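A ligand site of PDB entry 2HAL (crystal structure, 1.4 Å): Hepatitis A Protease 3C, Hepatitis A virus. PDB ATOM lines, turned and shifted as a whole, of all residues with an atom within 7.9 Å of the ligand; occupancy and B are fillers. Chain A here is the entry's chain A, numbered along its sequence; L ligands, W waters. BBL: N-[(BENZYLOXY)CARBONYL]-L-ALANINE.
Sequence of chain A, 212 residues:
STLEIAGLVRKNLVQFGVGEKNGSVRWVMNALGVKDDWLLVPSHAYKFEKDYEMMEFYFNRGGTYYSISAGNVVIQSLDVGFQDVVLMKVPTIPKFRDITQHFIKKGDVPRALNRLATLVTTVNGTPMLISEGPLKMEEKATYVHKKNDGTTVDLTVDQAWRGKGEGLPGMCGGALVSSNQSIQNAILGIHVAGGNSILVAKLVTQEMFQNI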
ATOM      1  N   GLU A   4      14.705   7.755 -32.994  1.00  0.00           N
ATOM      2  CA  GLU A   4      14.277   8.135 -31.649  1.00  0.00           C
ATOM      3  C   GLU A   4      13.261   7.144 -31.082  1.00  0.00           C
ATOM      4  O   GLU A   4      13.320   6.805 -29.900  1.00  0.00           O
ATOM      5  CB  GLU A   4      13.769   9.582 -31.595  1.00  0.00           C
ATOM      6  CG  GLU A   4      14.831  10.653 -31.905  1.00  0.00           C
ATOM      7  CD  GLU A   4      15.956  10.738 -30.867  1.00  0.00           C
ATOM      8  OE1 GLU A   4      15.727  10.418 -29.680  1.00  0.00           O
ATOM      9  OE2 GLU A   4      17.074  11.146 -31.245  1.00  0.00           O
ATOM     10  N   ILE A   5      12.352   6.636 -31.913  1.00  0.00           N
ATOM     11  CA  ILE A   5      11.473   5.543 -31.469  1.00  0.00           C
ATOM     12  C   ILE A   5      12.312   4.318 -31.129  1.00  0.00           C
ATOM     13  O   ILE A   5      12.053   3.653 -30.135  1.00  0.00           O
ATOM     14  CB  ILE A   5      10.430   5.145 -32.550  1.00  0.00           C
ATOM     15  CG1 ILE A   5       9.412   6.263 -32.729  1.00  0.00           C
ATOM     16  CG2 ILE A   5       9.732   3.827 -32.183  1.00  0.00           C
ATOM     17  CD1 ILE A   5       8.405   6.431 -31.582  1.00  0.00           C
ATOM     18  N   LEU A   8      13.686   4.441 -27.697  1.00  0.00           N
ATOM     19  CA  LEU A   8      12.688   4.174 -26.671  1.00  0.00           C
ATOM     20  C   LEU A   8      12.406   2.682 -26.562  1.00  0.00           C
ATOM     21  O   LEU A   8      12.223   2.166 -25.464  1.00  0.00           O
ATOM     22  CB  LEU A   8      11.395   4.913 -26.958  1.00  0.00           C
ATOM     23  CG  LEU A   8      11.464   6.437 -26.965  1.00  0.00           C
ATOM     24  CD1 LEU A   8      10.082   6.962 -27.230  1.00  0.00           C
ATOM     25  CD2 LEU A   8      12.026   7.001 -25.660  1.00  0.00           C
ATOM     26  N   ARG A  97       9.132   2.773 -18.546  1.00  0.00           N
ATOM     27  CA  ARG A  97       8.564   3.931 -19.250  1.00  0.00           C
ATOM     28  C   ARG A  97       7.375   3.472 -20.104  1.00  0.00           C
ATOM     29  O   ARG A  97       7.503   2.490 -20.825  1.00  0.00           O
ATOM     30  CB  ARG A  97       9.606   4.570 -20.157  1.00  0.00           C
ATOM     31  CG  ARG A  97       9.095   5.750 -20.983  1.00  0.00           C
ATOM     32  CD  ARG A  97      10.181   6.382 -21.812  1.00  0.00           C
ATOM     33  NE  ARG A  97       9.766   7.652 -22.374  1.00  0.00           N
ATOM     34  CZ  ARG A  97      10.611   8.605 -22.756  1.00  0.00           C
ATOM     35  NH1 ARG A  97      11.917   8.424 -22.625  1.00  0.00           N
ATOM     36  NH2 ARG A  97      10.151   9.739 -23.270  1.00  0.00           N
ATOM     37  N   ASP A  98       6.260   4.195 -20.006  1.00  0.00           N
ATOM     38  CA  ASP A  98       5.051   3.897 -20.757  1.00  0.00           C
ATOM     39  C   ASP A  98       5.285   4.260 -22.220  1.00  0.00           C
ATOM     40  O   ASP A  98       5.430   5.441 -22.559  1.00  0.00           O
ATOM     41  CB  ASP A  98       3.860   4.682 -20.182  1.00  0.00           C
ATOM     42  CG  ASP A  98       2.525   4.366 -20.852  1.00  0.00           C
ATOM     43  OD1 ASP A  98       2.465   3.620 -21.859  1.00  0.00           O
ATOM     44  OD2 ASP A  98       1.507   4.904 -20.379  1.00  0.00           O
ATOM     45  N   ILE A  99       5.328   3.246 -23.083  1.00  0.00           N
ATOM     46  CA  ILE A  99       5.515   3.488 -24.514  1.00  0.00           C
ATOM     47  C   ILE A  99       4.274   3.113 -25.310  1.00  0.00           C
ATOM     48  O   ILE A  99       4.306   3.073 -26.541  1.00  0.00           O
ATOM     49  CB  ILE A  99       6.792   2.787 -25.080  1.00  0.00           C
ATOM     50  CG1 ILE A  99       6.793   1.264 -24.825  1.00  0.00           C
ATOM     51  CG2 ILE A  99       8.055   3.450 -24.531  1.00  0.00           C
ATOM     52  CD1 ILE A  99       7.870   0.526 -25.592  1.00  0.00           C
ATOM     53  N   THR A 100       3.157   2.863 -24.618  1.00  0.00           N
ATOM     54  CA  THR A 100       1.959   2.368 -25.287  1.00  0.00           C
ATOM     55  C   THR A 100       1.404   3.341 -26.326  1.00  0.00           C
ATOM     56  O   THR A 100       0.768   2.940 -27.314  1.00  0.00           O
ATOM     57  CB  THR A 100       0.829   2.015 -24.294  1.00  0.00           C
ATOM     58  OG1 THR A 100       0.505   3.177 -23.522  1.00  0.00           O
ATOM     59  CG2 THR A 100       1.235   0.870 -23.379  1.00  0.00           C
ATOM     60  N   GLN A 101       1.652   4.628 -26.118  1.00  0.00           N
ATOM     61  CA  GLN A 101       1.115   5.649 -27.014  1.00  0.00           C
ATOM     62  C   GLN A 101       1.916   5.755 -28.310  1.00  0.00           C
ATOM     63  O   GLN A 101       1.526   6.460 -29.244  1.00  0.00           O
ATOM     64  CB  GLN A 101       0.986   7.000 -26.303  1.00  0.00           C
ATOM     65  CG  GLN A 101       0.213   6.910 -25.004  1.00  0.00           C
ATOM     66  CD  GLN A 101      -1.184   6.349 -25.201  1.00  0.00           C
ATOM     67  OE1 GLN A 101      -1.512   5.262 -24.733  1.00  0.00           O
ATOM     68  NE2 GLN A 101      -2.001   7.085 -25.924  1.00  0.00           N
ATOM     69  N   HIS A 102       3.048   5.046 -28.363  1.00  0.00           N
ATOM     70  CA  HIS A 102       3.873   4.997 -29.564  1.00  0.00           C
ATOM     71  C   HIS A 102       3.510   3.827 -30.480  1.00  0.00           C
ATOM     72  O   HIS A 102       4.063   3.726 -31.579  1.00  0.00           O
ATOM     73  CB  HIS A 102       5.362   4.949 -29.192  1.00  0.00           C
ATOM     74  CG  HIS A 102       5.863   6.231 -28.605  1.00  0.00           C
ATOM     75  ND1 HIS A 102       5.977   7.386 -29.355  1.00  0.00           N
ATOM     76  CD2 HIS A 102       6.221   6.565 -27.341  1.00  0.00           C
ATOM     77  CE1 HIS A 102       6.413   8.367 -28.575  1.00  0.00           C
ATOM     78  NE2 HIS A 102       6.571   7.893 -27.359  1.00  0.00           N
HETATM   79  OG2 BBL L   1       7.626   9.429 -23.605  1.00  0.00           O
HETATM   80  CB2 BBL L   1       6.680   9.941 -24.242  1.00  0.00           C
HETATM   81  OG1 BBL L   1       6.195  11.074 -23.941  1.00  0.00           O
HETATM   82  CA  BBL L   1       6.078   9.156 -25.389  1.00  0.00           C
HETATM   83  CBZ BBL L   1       7.145   8.619 -26.350  1.00  0.00           C
HETATM   84  N   BBL L   1       5.129   9.942 -26.138  1.00  0.00           N
HETATM   85  C   BBL L   1       3.897  10.176 -25.698  1.00  0.00           C
HETATM   86  O   BBL L   1       3.317   9.511 -24.841  1.00  0.00           O
HETATM   87  OEZ BBL L   1       3.250  11.294 -26.329  1.00  0.00           O
HETATM   88  CB  BBL L   1       1.860  11.553 -26.163  1.00  0.00           C
HETATM   89  CG  BBL L   1       1.586  12.924 -26.728  1.00  0.00           C
HETATM   90  CD1 BBL L   1       0.263  13.355 -26.815  1.00  0.00           C
HETATM   91  CE1 BBL L   1      -0.002  14.610 -27.341  1.00  0.00           C
HETATM   92  CZ  BBL L   1       1.038  15.426 -27.766  1.00  0.00           C
HETATM   93  CE2 BBL L   1       2.358  14.993 -27.692  1.00  0.00           C
HETATM   94  CD2 BBL L   1       2.638  13.742 -27.171  1.00  0.00           C
HETATM   95  O   HOH W   1      -1.312  10.077 -26.148  1.00  0.00           O
HETATM   96  O   HOH W   2       8.302  11.235 -21.775  1.00  0.00           O
HETATM   97  O   HOH W   3       5.182  10.104 -21.594  1.00  0.00           O
HETATM   98  O   HOH W   4       3.348   6.228 -24.262  1.00  0.00           O
HETATM   99  O   HOH W   5       1.421   8.862 -22.552  1.00  0.00           O
HETATM  100  O   HOH W   6       7.264   6.893 -23.507  1.00  0.00           O
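The side-chain hydroxyl of Thr 100 is in hydrogen-bond range of the side-chain amide oxygen of Gln 101 (3.1 Å).
Water W6 lies within hydrogen-bond range of O of Asp 98 (2.5 Å), OG2 of the ligand (2.6 Å) and NE of Arg 97 (2.8 Å). Water W2 bridges an oxygen (OG2) of the ligand (2.7 Å) and the guanidinium group (NH2) of Arg 97 (2.8 Å). Water W4 lies within hydrogen-bond range of the backbone carbonyl oxygen (O) of Asp 98 (2.8 Å), the backbone NH (N) of Gln 101 (3.0 Å), an oxygen (O) of the ligand (3.3 Å) and the backbone NH (N) of Thr 100 (3.4 Å).
Leu 8 touches the ligand. Gln 101 touches the ligand. Hydrophobic or aromatic side chains that line the ligand: Leu 8 and His 102.
OG2 of the ligand lies within salt-bridge range of NH2 of Arg 97, at 2.6 Å. NE2 of His 102 is covalently linked to CBZ of the ligand, 1.4 Å away.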
